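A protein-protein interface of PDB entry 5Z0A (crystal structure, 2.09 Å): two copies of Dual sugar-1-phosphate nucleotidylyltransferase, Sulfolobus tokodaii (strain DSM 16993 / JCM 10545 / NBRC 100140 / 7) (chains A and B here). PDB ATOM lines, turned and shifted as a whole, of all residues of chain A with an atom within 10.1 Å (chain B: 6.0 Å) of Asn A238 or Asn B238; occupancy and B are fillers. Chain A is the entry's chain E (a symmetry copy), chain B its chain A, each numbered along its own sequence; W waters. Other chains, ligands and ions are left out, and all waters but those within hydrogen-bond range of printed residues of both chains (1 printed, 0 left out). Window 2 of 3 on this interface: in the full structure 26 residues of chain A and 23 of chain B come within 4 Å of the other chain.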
ATOM      1  N   VAL A 235     -13.802 -12.266  -0.030  1.00  0.00           N
ATOM      2  CA  VAL A 235     -14.799 -11.824   0.931  1.00  0.00           C
ATOM      3  C   VAL A 235     -15.563 -13.029   1.450  1.00  0.00           C
ATOM      4  O   VAL A 235     -16.206 -13.734   0.696  1.00  0.00           O
ATOM      5  CB  VAL A 235     -15.743 -10.829   0.295  1.00  0.00           C
ATOM      6  CG1 VAL A 235     -16.735 -10.301   1.299  1.00  0.00           C
ATOM      7  CG2 VAL A 235     -14.938  -9.704  -0.357  1.00  0.00           C
ATOM      8  N   GLU A 236     -15.484 -13.265   2.751  1.00  0.00           N
ATOM      9  CA  GLU A 236     -16.242 -14.363   3.396  1.00  0.00           C
ATOM     10  C   GLU A 236     -17.713 -14.054   3.425  1.00  0.00           C
ATOM     11  O   GLU A 236     -18.101 -12.893   3.207  1.00  0.00           O
ATOM     12  CB  GLU A 236     -15.708 -14.628   4.828  1.00  0.00           C
ATOM     13  CG  GLU A 236     -14.310 -15.236   4.754  1.00  0.00           C
ATOM     14  CD  GLU A 236     -13.711 -15.578   6.079  1.00  0.00           C
ATOM     15  OE1 GLU A 236     -14.196 -15.129   7.154  1.00  0.00           O
ATOM     16  OE2 GLU A 236     -12.697 -16.296   6.047  1.00  0.00           O
ATOM     17  N   ASP A 237     -18.540 -15.042   3.798  1.00  0.00           N
ATOM     18  CA  ASP A 237     -19.951 -14.715   4.098  1.00  0.00           C
ATOM     19  C   ASP A 237     -20.142 -13.872   5.369  1.00  0.00           C
ATOM     20  O   ASP A 237     -19.214 -13.723   6.168  1.00  0.00           O
ATOM     21  CB  ASP A 237     -20.971 -15.870   4.048  1.00  0.00           C
ATOM     22  CG  ASP A 237     -20.450 -17.130   4.554  1.00  0.00           C
ATOM     23  OD1 ASP A 237     -19.842 -17.093   5.655  1.00  0.00           O
ATOM     24  OD2 ASP A 237     -20.657 -18.149   3.819  1.00  0.00           O
ATOM     25  N   ASN A 238     -21.309 -13.229   5.430  1.00  0.00           N
ATOM     26  CA  ASN A 238     -21.700 -12.337   6.500  1.00  0.00           C
ATOM     27  C   ASN A 238     -20.800 -11.134   6.538  1.00  0.00           C
ATOM     28  O   ASN A 238     -20.457 -10.621   7.626  1.00  0.00           O
ATOM     29  CB  ASN A 238     -21.632 -13.044   7.870  1.00  0.00           C
ATOM     30  CG  ASN A 238     -22.866 -13.848   8.225  1.00  0.00           C
ATOM     31  OD1 ASN A 238     -23.057 -14.144   9.415  1.00  0.00           O
ATOM     32  ND2 ASN A 238     -23.726 -14.186   7.250  1.00  0.00           N
ATOM     33  N   VAL A 239     -20.374 -10.698   5.376  1.00  0.00           N
ATOM     34  CA  VAL A 239     -19.717  -9.396   5.243  1.00  0.00           C
ATOM     35  C   VAL A 239     -20.744  -8.439   4.617  1.00  0.00           C
ATOM     36  O   VAL A 239     -21.359  -8.736   3.615  1.00  0.00           O
ATOM     37  CB  VAL A 239     -18.441  -9.494   4.398  1.00  0.00           C
ATOM     38  CG1 VAL A 239     -17.854  -8.115   4.087  1.00  0.00           C
ATOM     39  CG2 VAL A 239     -17.401 -10.323   5.118  1.00  0.00           C
ATOM     40  N   LYS A 240     -20.891  -7.273   5.178  1.00  0.00           N
ATOM     41  CA  LYS A 240     -21.858  -6.350   4.647  1.00  0.00           C
ATOM     42  C   LYS A 240     -21.090  -5.208   3.982  1.00  0.00           C
ATOM     43  O   LYS A 240     -20.185  -4.578   4.606  1.00  0.00           O
ATOM     44  CB  LYS A 240     -22.805  -5.901   5.746  1.00  0.00           C
ATOM     45  CG  LYS A 240     -23.705  -4.731   5.354  1.00  0.00           C
ATOM     46  CD  LYS A 240     -24.534  -4.979   4.082  1.00  0.00           C
ATOM     47  CE  LYS A 240     -25.967  -4.466   4.183  1.00  0.00           C
ATOM     48  NZ  LYS A 240     -26.682  -5.007   5.389  1.00  0.00           N
ATOM     49  N   ILE A 241     -21.436  -4.952   2.715  1.00  0.00           N
ATOM     50  CA  ILE A 241     -20.789  -3.911   1.958  1.00  0.00           C
ATOM     51  C   ILE A 241     -21.848  -2.968   1.442  1.00  0.00           C
ATOM     52  O   ILE A 241     -22.720  -3.387   0.708  1.00  0.00           O
ATOM     53  CB  ILE A 241     -19.995  -4.497   0.804  1.00  0.00           C
ATOM     54  CG1 ILE A 241     -18.815  -5.312   1.336  1.00  0.00           C
ATOM     55  CG2 ILE A 241     -19.452  -3.388  -0.096  1.00  0.00           C
ATOM     56  CD1 ILE A 241     -18.116  -6.156   0.297  1.00  0.00           C
ATOM     57  N   ILE A 253     -11.216 -10.453   3.592  1.00  0.00           N
ATOM     58  CA  ILE A 253     -12.213  -9.830   4.458  1.00  0.00           C
ATOM     59  C   ILE A 253     -13.072 -10.885   5.168  1.00  0.00           C
ATOM     60  O   ILE A 253     -13.879 -11.611   4.529  1.00  0.00           O
ATOM     61  CB  ILE A 253     -13.075  -8.861   3.685  1.00  0.00           C
ATOM     62  CG1 ILE A 253     -12.166  -7.923   2.860  1.00  0.00           C
ATOM     63  CG2 ILE A 253     -13.967  -8.130   4.629  1.00  0.00           C
ATOM     64  CD1 ILE A 253     -12.895  -6.814   2.156  1.00  0.00           C
ATOM     65  N   LYS A 254     -12.947 -10.933   6.486  1.00  0.00           N
ATOM     66  CA  LYS A 254     -13.552 -12.007   7.283  1.00  0.00           C
ATOM     67  C   LYS A 254     -14.912 -11.644   7.792  1.00  0.00           C
ATOM     68  O   LYS A 254     -15.287 -10.452   7.917  1.00  0.00           O
ATOM     69  CB  LYS A 254     -12.675 -12.386   8.482  1.00  0.00           C
ATOM     70  CG  LYS A 254     -11.307 -12.854   8.049  1.00  0.00           C
ATOM     71  CD  LYS A 254     -10.437 -13.183   9.260  1.00  0.00           C
ATOM     72  CE  LYS A 254      -9.151 -13.835   8.794  1.00  0.00           C
ATOM     73  NZ  LYS A 254      -8.281 -14.037   9.980  1.00  0.00           N
ATOM     74  N   SER A 255     -15.691 -12.696   8.043  1.00  0.00           N
ATOM     75  CA  SER A 255     -17.122 -12.539   8.442  1.00  0.00           C
ATOM     76  C   SER A 255     -17.352 -11.508   9.543  1.00  0.00           C
ATOM     77  O   SER A 255     -16.569 -11.382  10.472  1.00  0.00           O
ATOM     78  CB  SER A 255     -17.672 -13.930   8.858  1.00  0.00           C
ATOM     79  OG  SER A 255     -17.512 -14.887   7.823  1.00  0.00           O
ATOM     80  N   GLY A 256     -18.513 -10.841   9.497  1.00  0.00           N
ATOM     81  CA  GLY A 256     -18.896  -9.879  10.496  1.00  0.00           C
ATOM     82  C   GLY A 256     -18.383  -8.483  10.186  1.00  0.00           C
ATOM     83  O   GLY A 256     -18.789  -7.548  10.839  1.00  0.00           O
ATOM     84  N   THR A 257     -17.453  -8.354   9.270  1.00  0.00           N
ATOM     85  CA  THR A 257     -16.998  -7.063   8.817  1.00  0.00           C
ATOM     86  C   THR A 257     -18.121  -6.310   8.134  1.00  0.00           C
ATOM     87  O   THR A 257     -18.914  -6.868   7.361  1.00  0.00           O
ATOM     88  CB  THR A 257     -15.790  -7.229   7.870  1.00  0.00           C
ATOM     89  OG1 THR A 257     -14.727  -7.786   8.621  1.00  0.00           O
ATOM     90  CG2 THR A 257     -15.335  -5.888   7.269  1.00  0.00           C
ATOM     91  N   TYR A 258     -18.171  -5.028   8.447  1.00  0.00           N
ATOM     92  CA  TYR A 258     -19.160  -4.133   7.971  1.00  0.00           C
ATOM     93  C   TYR A 258     -18.497  -2.952   7.339  1.00  0.00           C
ATOM     94  O   TYR A 258     -17.677  -2.260   7.991  1.00  0.00           O
ATOM     95  CB  TYR A 258     -20.051  -3.704   9.111  1.00  0.00           C
ATOM     96  CG  TYR A 258     -21.347  -3.041   8.728  1.00  0.00           C
ATOM     97  CD1 TYR A 258     -22.524  -3.782   8.624  1.00  0.00           C
ATOM     98  CD2 TYR A 258     -21.446  -1.668   8.546  1.00  0.00           C
ATOM     99  CE1 TYR A 258     -23.758  -3.154   8.299  1.00  0.00           C
ATOM    100  CE2 TYR A 258     -22.658  -1.033   8.264  1.00  0.00           C
ATOM    101  CZ  TYR A 258     -23.811  -1.766   8.179  1.00  0.00           C
ATOM    102  OH  TYR A 258     -24.993  -1.162   7.868  1.00  0.00           O
ATOM    103  N   ILE A 259     -18.870  -2.678   6.076  1.00  0.00           N
ATOM    104  CA  ILE A 259     -18.163  -1.637   5.271  1.00  0.00           C
ATOM    105  C   ILE A 259     -19.161  -0.648   4.675  1.00  0.00           C
ATOM    106  O   ILE A 259     -20.091  -1.053   3.958  1.00  0.00           O
ATOM    107  CB  ILE A 259     -17.326  -2.251   4.166  1.00  0.00           C
ATOM    108  CG1 ILE A 259     -16.351  -3.310   4.741  1.00  0.00           C
ATOM    109  CG2 ILE A 259     -16.575  -1.186   3.355  1.00  0.00           C
ATOM    110  CD1 ILE A 259     -15.588  -4.078   3.704  1.00  0.00           C
ATOM    111  N   ILE A 271      -8.643  -8.164   6.898  1.00  0.00           N
ATOM    112  CA  ILE A 271      -9.690  -7.439   7.591  1.00  0.00           C
ATOM    113  C   ILE A 271     -10.618  -8.382   8.328  1.00  0.00           C
ATOM    114  O   ILE A 271     -11.065  -9.375   7.739  1.00  0.00           O
ATOM    115  CB  ILE A 271     -10.520  -6.641   6.584  1.00  0.00           C
ATOM    116  CG1 ILE A 271      -9.658  -5.843   5.596  1.00  0.00           C
ATOM    117  CG2 ILE A 271     -11.485  -5.730   7.257  1.00  0.00           C
ATOM    118  CD1 ILE A 271      -8.807  -4.800   6.210  1.00  0.00           C
ATOM    119  N   GLY A 272     -10.931  -8.045   9.573  1.00  0.00           N
ATOM    120  CA  GLY A 272     -11.879  -8.736  10.382  1.00  0.00           C
ATOM    121  C   GLY A 272     -11.287  -9.858  11.192  1.00  0.00           C
ATOM    122  O   GLY A 272     -10.072 -10.002  11.270  1.00  0.00           O
ATOM    123  N   PRO A 273     -12.132 -10.690  11.793  1.00  0.00           N
ATOM    124  CA  PRO A 273     -13.580 -10.574  11.790  1.00  0.00           C
ATOM    125  C   PRO A 273     -14.071  -9.392  12.568  1.00  0.00           C
ATOM    126  O   PRO A 273     -13.339  -8.832  13.349  1.00  0.00           O
ATOM    127  CB  PRO A 273     -14.009 -11.866  12.496  1.00  0.00           C
ATOM    128  CG  PRO A 273     -12.937 -12.031  13.541  1.00  0.00           C
ATOM    129  CD  PRO A 273     -11.675 -11.692  12.795  1.00  0.00           C
ATOM    130  N   ASN A 274     -15.339  -9.058  12.358  1.00  0.00           N
ATOM    131  CA  ASN A 274     -15.996  -8.087  13.183  1.00  0.00           C
ATOM    132  C   ASN A 274     -15.291  -6.696  13.210  1.00  0.00           C
ATOM    133  O   ASN A 274     -15.148  -6.064  14.260  1.00  0.00           O
ATOM    134  CB  ASN A 274     -16.245  -8.694  14.581  1.00  0.00           C
ATOM    135  CG  ASN A 274     -17.050  -9.978  14.528  1.00  0.00           C
ATOM    136  OD1 ASN A 274     -17.921 -10.120  13.670  1.00  0.00           O
ATOM    137  ND2 ASN A 274     -16.733 -10.952  15.433  1.00  0.00           N
ATOM    138  N   SER A 275     -14.812  -6.265  12.036  1.00  0.00           N
ATOM    139  CA  SER A 275     -14.252  -4.946  11.800  1.00  0.00           C
ATOM    140  C   SER A 275     -15.300  -4.020  11.209  1.00  0.00           C
ATOM    141  O   SER A 275     -16.301  -4.500  10.634  1.00  0.00           O
ATOM    142  CB  SER A 275     -13.100  -5.024  10.794  1.00  0.00           C
ATOM    143  OG  SER A 275     -12.048  -5.790  11.289  1.00  0.00           O
ATOM    144  N   GLU B 236     -31.591  -4.119   9.388  1.00  0.00           N
ATOM    145  CA  GLU B 236     -30.799  -4.783   8.337  1.00  0.00           C
ATOM    146  C   GLU B 236     -30.792  -6.271   8.505  1.00  0.00           C
ATOM    147  O   GLU B 236     -31.142  -6.781   9.589  1.00  0.00           O
ATOM    148  CB  GLU B 236     -29.370  -4.216   8.307  1.00  0.00           C
ATOM    149  CG  GLU B 236     -29.374  -2.783   7.810  1.00  0.00           C
ATOM    150  CD  GLU B 236     -28.008  -2.146   7.713  1.00  0.00           C
ATOM    151  OE1 GLU B 236     -27.004  -2.668   8.233  1.00  0.00           O
ATOM    152  OE2 GLU B 236     -27.960  -1.071   7.087  1.00  0.00           O
ATOM    153  N   ASP B 237     -30.302  -7.001   7.507  1.00  0.00           N
ATOM    154  CA  ASP B 237     -30.011  -8.464   7.759  1.00  0.00           C
ATOM    155  C   ASP B 237     -28.872  -8.716   8.737  1.00  0.00           C
ATOM    156  O   ASP B 237     -28.078  -7.791   9.058  1.00  0.00           O
ATOM    157  CB  ASP B 237     -29.862  -9.382   6.513  1.00  0.00           C
ATOM    158  CG  ASP B 237     -29.222  -8.738   5.373  1.00  0.00           C
ATOM    159  OD1 ASP B 237     -28.154  -8.117   5.594  1.00  0.00           O
ATOM    160  OD2 ASP B 237     -29.799  -8.867   4.264  1.00  0.00           O
ATOM    161  N   ASN B 238     -28.863  -9.954   9.268  1.00  0.00           N
ATOM    162  CA  ASN B 238     -27.912 -10.376  10.281  1.00  0.00           C
ATOM    163  C   ASN B 238     -28.027  -9.547  11.551  1.00  0.00           C
ATOM    164  O   ASN B 238     -26.995  -9.266  12.216  1.00  0.00           O
ATOM    165  CB  ASN B 238     -26.438 -10.261   9.773  1.00  0.00           C
ATOM    166  CG  ASN B 238     -25.961 -11.455   8.963  1.00  0.00           C
ATOM    167  OD1 ASN B 238     -24.732 -11.608   8.807  1.00  0.00           O
ATOM    168  ND2 ASN B 238     -26.867 -12.263   8.399  1.00  0.00           N
ATOM    169  N   VAL B 239     -29.259  -9.169  11.888  1.00  0.00           N
ATOM    170  CA  VAL B 239     -29.568  -8.662  13.179  1.00  0.00           C
ATOM    171  C   VAL B 239     -30.268  -9.750  13.984  1.00  0.00           C
ATOM    172  O   VAL B 239     -31.177 -10.392  13.488  1.00  0.00           O
ATOM    173  CB  VAL B 239     -30.421  -7.401  13.061  1.00  0.00           C
ATOM    174  CG1 VAL B 239     -30.877  -6.949  14.441  1.00  0.00           C
ATOM    175  CG2 VAL B 239     -29.581  -6.280  12.440  1.00  0.00           C
ATOM    176  N   LYS B 240     -29.830 -10.004  15.204  1.00  0.00           N
ATOM    177  CA  LYS B 240     -30.404 -11.075  15.951  1.00  0.00           C
ATOM    178  C   LYS B 240     -31.223 -10.457  17.093  1.00  0.00           C
ATOM    179  O   LYS B 240     -30.731  -9.568  17.819  1.00  0.00           O
ATOM    180  CB  LYS B 240     -29.345 -12.049  16.420  1.00  0.00           C
ATOM    181  CG  LYS B 240     -29.837 -13.050  17.453  1.00  0.00           C
ATOM    182  CD  LYS B 240     -31.041 -13.876  16.985  1.00  0.00           C
ATOM    183  CE  LYS B 240     -30.959 -15.350  17.386  1.00  0.00           C
ATOM    184  NZ  LYS B 240     -29.678 -15.981  16.939  1.00  0.00           N
ATOM    185  N   LYS B 254     -28.256  -1.753  12.395  1.00  0.00           N
ATOM    186  CA  LYS B 254     -27.332  -2.313  11.410  1.00  0.00           C
ATOM    187  C   LYS B 254     -26.907  -3.705  11.678  1.00  0.00           C
ATOM    188  O   LYS B 254     -26.843  -4.144  12.862  1.00  0.00           O
ATOM    189  CB  LYS B 254     -26.108  -1.423  11.265  1.00  0.00           C
ATOM    190  CG  LYS B 254     -26.484  -0.006  10.869  1.00  0.00           C
ATOM    191  CD  LYS B 254     -25.274   0.932  10.780  1.00  0.00           C
ATOM    192  CE  LYS B 254     -25.683   2.290  10.200  1.00  0.00           C
ATOM    193  NZ  LYS B 254     -24.498   3.181  10.230  1.00  0.00           N
ATOM    194  N   SER B 255     -26.443  -4.370  10.624  1.00  0.00           N
ATOM    195  CA  SER B 255     -25.995  -5.812  10.680  1.00  0.00           C
ATOM    196  C   SER B 255     -24.994  -6.116  11.800  1.00  0.00           C
ATOM    197  O   SER B 255     -24.154  -5.307  12.169  1.00  0.00           O
ATOM    198  CB  SER B 255     -25.383  -6.244   9.319  1.00  0.00           C
ATOM    199  OG  SER B 255     -26.323  -5.982   8.255  1.00  0.00           O
ATOM    200  N   GLY B 256     -25.109  -7.325  12.377  1.00  0.00           N
ATOM    201  CA  GLY B 256     -24.242  -7.733  13.451  1.00  0.00           C
ATOM    202  C   GLY B 256     -24.764  -7.353  14.809  1.00  0.00           C
ATOM    203  O   GLY B 256     -24.238  -7.845  15.803  1.00  0.00           O
ATOM    204  N   THR B 257     -25.751  -6.474  14.888  1.00  0.00           N
ATOM    205  CA  THR B 257     -26.359  -6.132  16.164  1.00  0.00           C
ATOM    206  C   THR B 257     -27.073  -7.315  16.737  1.00  0.00           C
ATOM    207  O   THR B 257     -27.758  -8.060  16.012  1.00  0.00           O
ATOM    208  CB  THR B 257     -27.288  -4.936  16.011  1.00  0.00           C
ATOM    209  OG1 THR B 257     -26.496  -3.797  15.649  1.00  0.00           O
ATOM    210  CG2 THR B 257     -28.049  -4.607  17.322  1.00  0.00           C
HETATM  211  O   HOH W   1     -29.555  -5.526   5.166  1.00  0.00           O
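The side-chain carboxylate (OE1) of Glu B236 lies within hydrogen-bond range of the backbone NH (N) of Ser B255.
The backbone carbonyl oxygen (O) of Asp B237 is in hydrogen-bond range of the side-chain hydroxyl (OG) of Ser B255, 2.6 Å away.
O of Asn B238 sits at hydrogen-bond distance from N of Gly B256.
O of Lys B254 is in hydrogen-bond range of OG1 of Thr B257 (2.8 Å).
O of Thr A257 lies within hydrogen-bond range of N of Lys A240.
N of Tyr A258 lies within hydrogen-bond range of O of Ser A275 (2.9 Å).
Among the printed residues, pairs that only touch across the chains: Tyr A258 with Lys B254 (3.5 Å) and Tyr A258 with Ser B255 (3.6 Å).
Asn A238 touches its own counterpart, Asn B238.
Lys A240 touches Glu B236, but with the chains exchanged Glu A236 does not touch Lys B240 (17.0 Å).
Lys A240 touches Asp B237, but with the chains exchanged Asp A237 does not touch Lys B240 (14.3 Å).
Lys A240 touches Ser B255, but with the chains exchanged Ser A255 does not touch Lys B240 (13.8 Å).
Of the 7 pairs that touch across the chains among the printed residues, 1 has its exchanged pair printed and touching as well.
Water W1 bridges N of Asp B237 and NZ of Lys A240.
Of the 19 printed residues of chain A, 3 touch a printed residue of chain B.
Hydrophobic or aromatic side chains of chain A that line the printed part of chain B: Tyr A258.
Along chain A the printed residues that touch a printed residue of chain B span positions 238 to 258.
Printed residues of chain B that touch a printed residue of chain A: Glu B236, Asp B237, Asn B238, Lys B254 and Ser B255.
Among the printed residues, 7 pairs touch across the chains.
Of chain B, only Asn B238 (3.0 Å) comes within 4 Å of Asn A238.
Ile A253 touches none of the printed residues of chain B.
Ser A255 touches none of the printed residues of chain B.
Printed residues of chain B within 4 Å of Tyr A258: Glu B236 (2.5 Å), Lys B254 (3.5 Å) and Ser B255 (3.6 Å).
Of the printed residues of chain A, Glu B236 touches Lys A240 and Tyr A258.
Asp B237 touches just one residue of chain A: Lys A240 (3.4 Å).
Asn B238 touches just one residue of chain A: Asn A238.
No residue of chain A comes within 4 Å of Val B239.
Of the printed residues of chain A, Lys B254 touches Tyr A258.
Ser B255 touches just these residues of chain A: Lys A240 and Tyr A258.
No residue of chain A comes within 4 Å of Gly B256.
The nearest printed residue of chain A that does not touch Lys B254 is Lys A240 (6.4 Å).
The side-chain amino group (NZ) of Lys A240 lies within salt-bridge range of the side-chain carboxylate (OE1) of Glu B236 (3.7 Å).
The side-chain carboxylate of Glu B236 lies within hydrogen-bond range of the side-chain hydroxyl of Tyr A258, at 2.5 Å.
NZ of Lys A240 is in salt-bridge range of OD1 of Asp B237, at 3.4 Å.
The side-chain amide oxygen (OD1) of Asn B238 sits close to the side-chain amide oxygen (OD1) of Asn A238.
The side-chain amino group (NZ) of Lys A240 sits at hydrogen-bond distance from the side-chain hydroxyl (OG) of Ser B255, at 3.0 Å.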
